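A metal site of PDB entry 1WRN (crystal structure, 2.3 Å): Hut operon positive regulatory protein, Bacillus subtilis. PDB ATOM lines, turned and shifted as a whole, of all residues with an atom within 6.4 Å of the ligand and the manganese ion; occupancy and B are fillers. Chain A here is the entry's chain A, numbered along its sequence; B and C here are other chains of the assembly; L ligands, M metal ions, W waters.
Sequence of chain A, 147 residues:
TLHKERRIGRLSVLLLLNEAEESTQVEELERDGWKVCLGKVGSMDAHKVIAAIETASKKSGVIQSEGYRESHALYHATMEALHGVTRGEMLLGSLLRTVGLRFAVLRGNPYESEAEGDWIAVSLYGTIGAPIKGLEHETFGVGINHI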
ATOM      1  N   GLU A  54      26.894  14.595  -8.902  1.00  0.00           N
ATOM      2  CA  GLU A  54      27.477  15.389  -7.817  1.00  0.00           C
ATOM      3  C   GLU A  54      28.909  14.995  -7.462  1.00  0.00           C
ATOM      4  O   GLU A  54      29.734  15.860  -7.194  1.00  0.00           O
ATOM      5  CB  GLU A  54      26.615  15.292  -6.550  1.00  0.00           C
ATOM      6  CG  GLU A  54      27.283  15.921  -5.341  1.00  0.00           C
ATOM      7  CD  GLU A  54      26.405  15.899  -4.100  1.00  0.00           C
ATOM      8  OE1 GLU A  54      25.582  14.988  -3.945  1.00  0.00           O
ATOM      9  OE2 GLU A  54      26.562  16.795  -3.242  1.00  0.00           O
ATOM     10  N   TYR A  68      27.689  24.580   1.163  1.00  0.00           N
ATOM     11  CA  TYR A  68      26.415  24.172   0.593  1.00  0.00           C
ATOM     12  C   TYR A  68      26.105  24.887  -0.728  1.00  0.00           C
ATOM     13  O   TYR A  68      25.758  24.247  -1.729  1.00  0.00           O
ATOM     14  CB  TYR A  68      25.308  24.440   1.608  1.00  0.00           C
ATOM     15  CG  TYR A  68      23.950  23.911   1.234  1.00  0.00           C
ATOM     16  CD1 TYR A  68      23.793  22.630   0.689  1.00  0.00           C
ATOM     17  CD2 TYR A  68      22.795  24.661   1.469  1.00  0.00           C
ATOM     18  CE1 TYR A  68      22.540  22.112   0.398  1.00  0.00           C
ATOM     19  CE2 TYR A  68      21.536  24.153   1.186  1.00  0.00           C
ATOM     20  CZ  TYR A  68      21.416  22.888   0.652  1.00  0.00           C
ATOM     21  OH  TYR A  68      20.164  22.378   0.376  1.00  0.00           O
ATOM     22  N   SER A  71      26.686  23.257  -3.979  1.00  0.00           N
ATOM     23  CA  SER A  71      26.009  21.975  -4.011  1.00  0.00           C
ATOM     24  C   SER A  71      24.538  22.246  -4.255  1.00  0.00           C
ATOM     25  O   SER A  71      23.895  21.591  -5.060  1.00  0.00           O
ATOM     26  CB  SER A  71      26.195  21.219  -2.692  1.00  0.00           C
ATOM     27  OG  SER A  71      27.385  20.438  -2.717  1.00  0.00           O
ATOM     28  N   HIS A  72      23.989  23.246  -3.569  1.00  0.00           N
ATOM     29  CA  HIS A  72      22.585  23.576  -3.768  1.00  0.00           C
ATOM     30  C   HIS A  72      22.358  23.932  -5.240  1.00  0.00           C
ATOM     31  O   HIS A  72      21.368  23.518  -5.846  1.00  0.00           O
ATOM     32  CB  HIS A  72      22.184  24.716  -2.845  1.00  0.00           C
ATOM     33  CG  HIS A  72      20.729  25.053  -2.909  1.00  0.00           C
ATOM     34  ND1 HIS A  72      20.236  26.142  -3.600  1.00  0.00           N
ATOM     35  CD2 HIS A  72      19.659  24.474  -2.310  1.00  0.00           C
ATOM     36  CE1 HIS A  72      18.940  26.222  -3.422  1.00  0.00           C
ATOM     37  NE2 HIS A  72      18.558  25.215  -2.646  1.00  0.00           N
ATOM     38  N   TYR A  75      22.416  20.811  -7.426  1.00  0.00           N
ATOM     39  CA  TYR A  75      21.274  19.953  -7.124  1.00  0.00           C
ATOM     40  C   TYR A  75      20.015  20.366  -7.864  1.00  0.00           C
ATOM     41  O   TYR A  75      19.348  19.535  -8.471  1.00  0.00           O
ATOM     42  CB  TYR A  75      20.987  19.925  -5.624  1.00  0.00           C
ATOM     43  CG  TYR A  75      19.820  19.023  -5.278  1.00  0.00           C
ATOM     44  CD1 TYR A  75      20.024  17.651  -5.039  1.00  0.00           C
ATOM     45  CD2 TYR A  75      18.515  19.514  -5.217  1.00  0.00           C
ATOM     46  CE1 TYR A  75      18.955  16.809  -4.746  1.00  0.00           C
ATOM     47  CE2 TYR A  75      17.431  18.663  -4.926  1.00  0.00           C
ATOM     48  CZ  TYR A  75      17.665  17.309  -4.684  1.00  0.00           C
ATOM     49  OH  TYR A  75      16.609  16.464  -4.377  1.00  0.00           O
ATOM     50  N   HIS A  76      19.656  21.647  -7.792  1.00  0.00           N
ATOM     51  CA  HIS A  76      18.454  22.079  -8.484  1.00  0.00           C
ATOM     52  C   HIS A  76      18.627  21.986  -9.997  1.00  0.00           C
ATOM     53  O   HIS A  76      17.668  21.677 -10.723  1.00  0.00           O
ATOM     54  CB  HIS A  76      18.062  23.492  -8.018  1.00  0.00           C
ATOM     55  CG  HIS A  76      17.390  23.502  -6.674  1.00  0.00           C
ATOM     56  ND1 HIS A  76      16.093  23.087  -6.496  1.00  0.00           N
ATOM     57  CD2 HIS A  76      17.863  23.809  -5.442  1.00  0.00           C
ATOM     58  CE1 HIS A  76      15.793  23.128  -5.208  1.00  0.00           C
ATOM     59  NE2 HIS A  76      16.849  23.570  -4.547  1.00  0.00           N
ATOM     60  N   VAL B  85       6.692  21.454   1.647  1.00  0.00           N
ATOM     61  CA  VAL B  85       7.991  20.905   2.028  1.00  0.00           C
ATOM     62  C   VAL B  85       8.783  20.369   0.839  1.00  0.00           C
ATOM     63  O   VAL B  85       9.972  20.674   0.716  1.00  0.00           O
ATOM     64  CB  VAL B  85       7.820  19.765   3.079  1.00  0.00           C
ATOM     65  CG1 VAL B  85       9.172  19.170   3.469  1.00  0.00           C
ATOM     66  CG2 VAL B  85       7.125  20.288   4.311  1.00  0.00           C
ATOM     67  N   THR B  86       8.145  19.580  -0.026  1.00  0.00           N
ATOM     68  CA  THR B  86       8.842  19.005  -1.172  1.00  0.00           C
ATOM     69  C   THR B  86       8.869  19.888  -2.418  1.00  0.00           C
ATOM     70  O   THR B  86       9.741  19.747  -3.266  1.00  0.00           O
ATOM     71  CB  THR B  86       8.270  17.621  -1.550  1.00  0.00           C
ATOM     72  OG1 THR B  86       6.871  17.721  -1.771  1.00  0.00           O
ATOM     73  CG2 THR B  86       8.520  16.615  -0.440  1.00  0.00           C
ATOM     74  N   ARG B  87       7.904  20.792  -2.528  1.00  0.00           N
ATOM     75  CA  ARG B  87       7.826  21.719  -3.664  1.00  0.00           C
ATOM     76  C   ARG B  87       7.960  21.054  -5.046  1.00  0.00           C
ATOM     77  O   ARG B  87       8.929  21.294  -5.770  1.00  0.00           O
ATOM     78  CB  ARG B  87       8.905  22.803  -3.510  1.00  0.00           C
ATOM     79  CG  ARG B  87       8.663  23.767  -2.341  1.00  0.00           C
ATOM     80  CD  ARG B  87       9.977  24.169  -1.671  1.00  0.00           C
ATOM     81  NE  ARG B  87      10.601  23.017  -1.033  1.00  0.00           N
ATOM     82  CZ  ARG B  87      11.876  22.670  -1.176  1.00  0.00           C
ATOM     83  NH1 ARG B  87      12.677  23.403  -1.948  1.00  0.00           N
ATOM     84  NH2 ARG B  87      12.350  21.585  -0.577  1.00  0.00           N
ATOM     85  N   LEU B  95      15.296  11.062  -4.036  1.00  0.00           N
ATOM     86  CA  LEU B  95      15.844  12.250  -4.669  1.00  0.00           C
ATOM     87  C   LEU B  95      17.083  12.713  -3.886  1.00  0.00           C
ATOM     88  O   LEU B  95      17.441  13.889  -3.878  1.00  0.00           O
ATOM     89  CB  LEU B  95      14.809  13.372  -4.710  1.00  0.00           C
ATOM     90  CG  LEU B  95      13.658  13.174  -5.705  1.00  0.00           C
ATOM     91  CD1 LEU B  95      12.887  14.489  -5.819  1.00  0.00           C
ATOM     92  CD2 LEU B  95      14.185  12.743  -7.080  1.00  0.00           C
ATOM     93  N   LEU B  96      17.722  11.760  -3.236  1.00  0.00           N
ATOM     94  CA  LEU B  96      18.924  12.014  -2.460  1.00  0.00           C
ATOM     95  C   LEU B  96      18.789  13.204  -1.530  1.00  0.00           C
ATOM     96  O   LEU B  96      19.666  14.041  -1.457  1.00  0.00           O
ATOM     97  CB  LEU B  96      20.122  12.224  -3.395  1.00  0.00           C
ATOM     98  CG  LEU B  96      21.507  11.940  -2.778  1.00  0.00           C
ATOM     99  CD1 LEU B  96      21.630  10.433  -2.544  1.00  0.00           C
ATOM    100  CD2 LEU B  96      22.618  12.417  -3.688  1.00  0.00           C
ATOM    101  N   ARG B  97      17.674  13.282  -0.825  1.00  0.00           N
ATOM    102  CA  ARG B  97      17.495  14.359   0.139  1.00  0.00           C
ATOM    103  C   ARG B  97      16.820  13.826   1.390  1.00  0.00           C
ATOM    104  O   ARG B  97      16.140  12.798   1.355  1.00  0.00           O
ATOM    105  CB  ARG B  97      16.702  15.540  -0.472  1.00  0.00           C
ATOM    106  CG  ARG B  97      15.264  15.271  -0.857  1.00  0.00           C
ATOM    107  CD  ARG B  97      14.635  16.572  -1.390  1.00  0.00           C
ATOM    108  NE  ARG B  97      13.320  16.365  -2.006  1.00  0.00           N
ATOM    109  CZ  ARG B  97      12.653  17.320  -2.657  1.00  0.00           C
ATOM    110  NH1 ARG B  97      13.158  18.534  -2.781  1.00  0.00           N
ATOM    111  NH2 ARG B  97      11.473  17.052  -3.191  1.00  0.00           N
ATOM    112  N   THR B  98      17.040  14.510   2.507  1.00  0.00           N
ATOM    113  CA  THR B  98      16.438  14.102   3.769  1.00  0.00           C
ATOM    114  C   THR B  98      15.826  15.304   4.487  1.00  0.00           C
ATOM    115  O   THR B  98      16.124  16.448   4.169  1.00  0.00           O
ATOM    116  CB  THR B  98      17.470  13.465   4.722  1.00  0.00           C
ATOM    117  OG1 THR B  98      16.787  12.888   5.846  1.00  0.00           O
ATOM    118  CG2 THR B  98      18.439  14.509   5.239  1.00  0.00           C
ATOM    119  N   ILE B 128      15.678  20.660   5.059  1.00  0.00           N
ATOM    120  CA  ILE B 128      15.686  19.716   3.951  1.00  0.00           C
ATOM    121  C   ILE B 128      17.039  19.883   3.250  1.00  0.00           C
ATOM    122  O   ILE B 128      17.399  20.975   2.834  1.00  0.00           O
ATOM    123  CB  ILE B 128      14.510  19.944   2.954  1.00  0.00           C
ATOM    124  CG1 ILE B 128      14.463  18.765   1.962  1.00  0.00           C
ATOM    125  CG2 ILE B 128      14.656  21.306   2.224  1.00  0.00           C
ATOM    126  CD1 ILE B 128      13.204  18.684   1.136  1.00  0.00           C
ATOM    127  N   GLY B 129      17.796  18.793   3.129  1.00  0.00           N
ATOM    128  CA  GLY B 129      19.081  18.909   2.469  1.00  0.00           C
ATOM    129  C   GLY B 129      19.585  17.519   2.152  1.00  0.00           C
ATOM    130  O   GLY B 129      18.794  16.597   2.064  1.00  0.00           O
ATOM    131  N   ALA B 130      20.902  17.352   2.005  1.00  0.00           N
ATOM    132  CA  ALA B 130      21.448  16.038   1.706  1.00  0.00           C
ATOM    133  C   ALA B 130      21.516  15.215   2.984  1.00  0.00           C
ATOM    134  O   ALA B 130      21.263  15.725   4.071  1.00  0.00           O
ATOM    135  CB  ALA B 130      22.839  16.178   1.117  1.00  0.00           C
ATOM    136  N   PRO B 131      21.817  13.912   2.878  1.00  0.00           N
ATOM    137  CA  PRO B 131      21.919  13.023   4.027  1.00  0.00           C
ATOM    138  C   PRO B 131      22.958  13.529   5.053  1.00  0.00           C
ATOM    139  O   PRO B 131      22.798  13.338   6.257  1.00  0.00           O
ATOM    140  CB  PRO B 131      22.307  11.685   3.385  1.00  0.00           C
ATOM    141  CG  PRO B 131      22.860  12.087   2.042  1.00  0.00           C
ATOM    142  CD  PRO B 131      21.898  13.142   1.638  1.00  0.00           C
ATOM    143  N   LEU B 135      24.890  20.454   5.016  1.00  0.00           N
ATOM    144  CA  LEU B 135      24.281  20.781   3.735  1.00  0.00           C
ATOM    145  C   LEU B 135      22.745  20.814   3.715  1.00  0.00           C
ATOM    146  O   LEU B 135      22.116  19.776   3.574  1.00  0.00           O
ATOM    147  CB  LEU B 135      24.758  19.772   2.697  1.00  0.00           C
ATOM    148  CG  LEU B 135      26.253  19.477   2.731  1.00  0.00           C
ATOM    149  CD1 LEU B 135      26.605  18.416   1.703  1.00  0.00           C
ATOM    150  CD2 LEU B 135      27.021  20.760   2.481  1.00  0.00           C
ATOM    151  N   GLU B 136      22.151  22.005   3.825  1.00  0.00           N
ATOM    152  CA  GLU B 136      20.697  22.101   3.823  1.00  0.00           C
ATOM    153  C   GLU B 136      20.201  23.497   4.092  1.00  0.00           C
ATOM    154  O   GLU B 136      20.977  24.385   4.439  1.00  0.00           O
ATOM    155  CB  GLU B 136      20.124  21.179   4.897  1.00  0.00           C
ATOM    156  CG  GLU B 136      20.313  21.705   6.307  1.00  0.00           C
ATOM    157  CD  GLU B 136      20.570  20.590   7.316  1.00  0.00           C
ATOM    158  OE1 GLU B 136      20.942  19.478   6.888  1.00  0.00           O
ATOM    159  OE2 GLU B 136      20.409  20.844   8.529  1.00  0.00           O
ATOM    160  N   HIS B 137      18.899  23.683   3.934  1.00  0.00           N
ATOM    161  CA  HIS B 137      18.258  24.954   4.232  1.00  0.00           C
ATOM    162  C   HIS B 137      16.886  24.689   4.834  1.00  0.00           C
ATOM    163  O   HIS B 137      16.525  23.541   5.072  1.00  0.00           O
ATOM    164  CB  HIS B 137      18.197  25.882   2.997  1.00  0.00           C
ATOM    165  CG  HIS B 137      17.448  25.325   1.824  1.00  0.00           C
ATOM    166  ND1 HIS B 137      16.091  25.108   1.833  1.00  0.00           N
ATOM    167  CD2 HIS B 137      17.862  25.027   0.570  1.00  0.00           C
ATOM    168  CE1 HIS B 137      15.695  24.711   0.634  1.00  0.00           C
ATOM    169  NE2 HIS B 137      16.757  24.658  -0.154  1.00  0.00           N
ATOM    170  N   GLU C  80       8.959  28.455  -5.561  1.00  0.00           N
ATOM    171  CA  GLU C  80       8.969  27.445  -4.517  1.00  0.00           C
ATOM    172  C   GLU C  80       7.959  27.797  -3.423  1.00  0.00           C
ATOM    173  O   GLU C  80       7.440  26.915  -2.756  1.00  0.00           O
ATOM    174  CB  GLU C  80      10.375  27.246  -3.944  1.00  0.00           C
ATOM    175  CG  GLU C  80      11.389  26.853  -5.036  1.00  0.00           C
ATOM    176  CD  GLU C  80      12.439  25.856  -4.579  1.00  0.00           C
ATOM    177  OE1 GLU C  80      12.436  25.466  -3.396  1.00  0.00           O
ATOM    178  N   TRP C 119      21.511  34.514   0.572  1.00  0.00           N
ATOM    179  CA  TRP C 119      20.411  33.641   0.203  1.00  0.00           C
ATOM    180  C   TRP C 119      19.180  34.544   0.249  1.00  0.00           C
ATOM    181  O   TRP C 119      19.206  35.625   0.849  1.00  0.00           O
ATOM    182  CB  TRP C 119      20.269  32.505   1.213  1.00  0.00           C
ATOM    183  CG  TRP C 119      21.345  31.494   1.083  1.00  0.00           C
ATOM    184  CD1 TRP C 119      22.665  31.674   1.368  1.00  0.00           C
ATOM    185  CD2 TRP C 119      21.212  30.161   0.604  1.00  0.00           C
ATOM    186  NE1 TRP C 119      23.372  30.527   1.088  1.00  0.00           N
ATOM    187  CE2 TRP C 119      22.501  29.580   0.623  1.00  0.00           C
ATOM    188  CE3 TRP C 119      20.121  29.399   0.164  1.00  0.00           C
ATOM    189  CZ2 TRP C 119      22.730  28.264   0.207  1.00  0.00           C
ATOM    190  CZ3 TRP C 119      20.357  28.091  -0.244  1.00  0.00           C
ATOM    191  CH2 TRP C 119      21.649  27.539  -0.220  1.00  0.00           C
ATOM    192  N   ILE C 144      13.072  29.199  -0.645  1.00  0.00           N
ATOM    193  CA  ILE C 144      14.436  29.522  -0.247  1.00  0.00           C
ATOM    194  C   ILE C 144      15.431  29.246  -1.367  1.00  0.00           C
ATOM    195  O   ILE C 144      15.465  28.134  -1.919  1.00  0.00           O
ATOM    196  CB  ILE C 144      14.803  28.698   1.025  1.00  0.00           C
ATOM    197  CG1 ILE C 144      13.964  29.187   2.206  1.00  0.00           C
ATOM    198  CG2 ILE C 144      16.294  28.803   1.326  1.00  0.00           C
ATOM    199  CD1 ILE C 144      14.307  28.533   3.507  1.00  0.00           C
ATOM    200  N   ASN C 145      16.230  30.246  -1.718  1.00  0.00           N
ATOM    201  CA  ASN C 145      17.210  30.076  -2.788  1.00  0.00           C
ATOM    202  C   ASN C 145      18.542  30.793  -2.518  1.00  0.00           C
ATOM    203  O   ASN C 145      18.576  31.739  -1.743  1.00  0.00           O
ATOM    204  CB  ASN C 145      16.624  30.606  -4.092  1.00  0.00           C
ATOM    205  CG  ASN C 145      17.275  29.983  -5.303  1.00  0.00           C
ATOM    206  OD1 ASN C 145      17.010  30.406  -6.433  1.00  0.00           O
ATOM    207  ND2 ASN C 145      18.124  28.972  -5.089  1.00  0.00           N
HETATM  208  C1  LIG L   1      17.083  20.773  -1.983  1.00  0.00           C
HETATM  209  C2  LIG L   1      15.611  21.140  -1.815  1.00  0.00           C
HETATM  210  O1  LIG L   1      15.257  22.318  -2.034  1.00  0.00           O
HETATM  211  C3  LIG L   1      17.457  19.697  -0.951  1.00  0.00           C
HETATM  212  C4  LIG L   1      18.844  19.151  -1.102  1.00  0.00           C
HETATM  213  N1  LIG L   1      19.962  19.870  -0.724  1.00  0.00           N
HETATM  214  C5  LIG L   1      19.288  17.955  -1.546  1.00  0.00           C
HETATM  215  C6  LIG L   1      21.037  19.121  -0.926  1.00  0.00           C
HETATM  216  N2  LIG L   1      20.655  17.961  -1.425  1.00  0.00           N
HETATM  217  O2  LIG L   1      14.806  20.233  -1.481  1.00  0.00           O
HETATM  218 MN    MN M   1      16.882  23.862  -2.282  1.00  0.00          MN
HETATM  219  O   HOH W   1      21.659  15.358  -2.173  1.00  0.00           O
HETATM  220  O   HOH W   2      15.676  25.488  -2.896  1.00  0.00           O
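O2 of the ligand lies within salt-bridge range of NH1 of Arg 97 of chain B. The backbone NH of Ala 130 of chain B lies close to a nitrogen (N2) of the ligand, 3.5 Å away. An oxygen (O2) of the ligand lies within salt-bridge range of the guanidinium group (NH2) of Arg 87 of chain B (2.9 Å). A nitrogen (N1) of the ligand is in hydrogen-bond range of the side-chain hydroxyl of Tyr 68, 2.7 Å away.
OH of Tyr 75 lies within hydrogen-bond range of O of Leu 95 of chain B, at 2.8 Å. The backbone carbonyl oxygen of His 137 of chain B is in hydrogen-bond range of the backbone NH of Ile 128 of chain B (3.0 Å). The backbone carbonyl oxygen (O) of Gly 129 of chain B lies within hydrogen-bond range of the backbone NH (N) of Thr 98 of chain B. NH2 of Arg 97 of chain B sits at hydrogen-bond distance from O of Thr 86 of chain B, at 3.2 Å. O of Leu 135 of chain B sits at hydrogen-bond distance from N of Ala 130 of chain B, 3.1 Å away. NH1 of Arg 87 of chain B lies within salt-bridge range of OE1 of Glu 80 of chain C, 2.5 Å away.
CE1 of Tyr 75 touches C5 of the ligand, at 3.4 Å. O of Leu 96 of chain B touches C5 of the ligand, 3.9 Å away. CD1 of Ile 128 of chain B touches O2 of the ligand, 3.4 Å away. Gly 129 of chain B touches the ligand. Within 4 Å of the ligand: Tyr 68, Tyr 75, His 76, Arg 87 of chain B, Leu 96 of chain B, Arg 97 of chain B, Ile 128 of chain B, Gly 129 of chain B, Ala 130 of chain B and His 137 of chain B. The nearest printed residue that does not touch the ligand is His 72 (4.4 Å).
Three residues have an atom within 4 Å of the manganese ion: His 72, His 76 and His 137 of chain B. The nearest printed residue that does not touch the manganese ion is Arg 87 of chain B (4.2 Å).
The manganese ion is bound by water W2 (2.1 Å), a ring nitrogen (NE2) of His 72 (2.2 Å), an oxygen (O1) of the ligand (2.3 Å), a ring nitrogen (NE2) of His 137 of chain B (2.3 Å) and a ring nitrogen (NE2) of His 76 (2.3 Å). The manganese ion has five donor atoms within binding distance.
Water W2 lies within hydrogen-bond range of O of Ile 144 of chain C (2.8 Å) and OE1 of Glu 80 of chain C (3.3 Å). Water W1 lies within hydrogen-bond range of the backbone carbonyl oxygen (O) of Leu 96 of chain B (2.5 Å) and a nitrogen (N2) of the ligand (2.9 Å).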
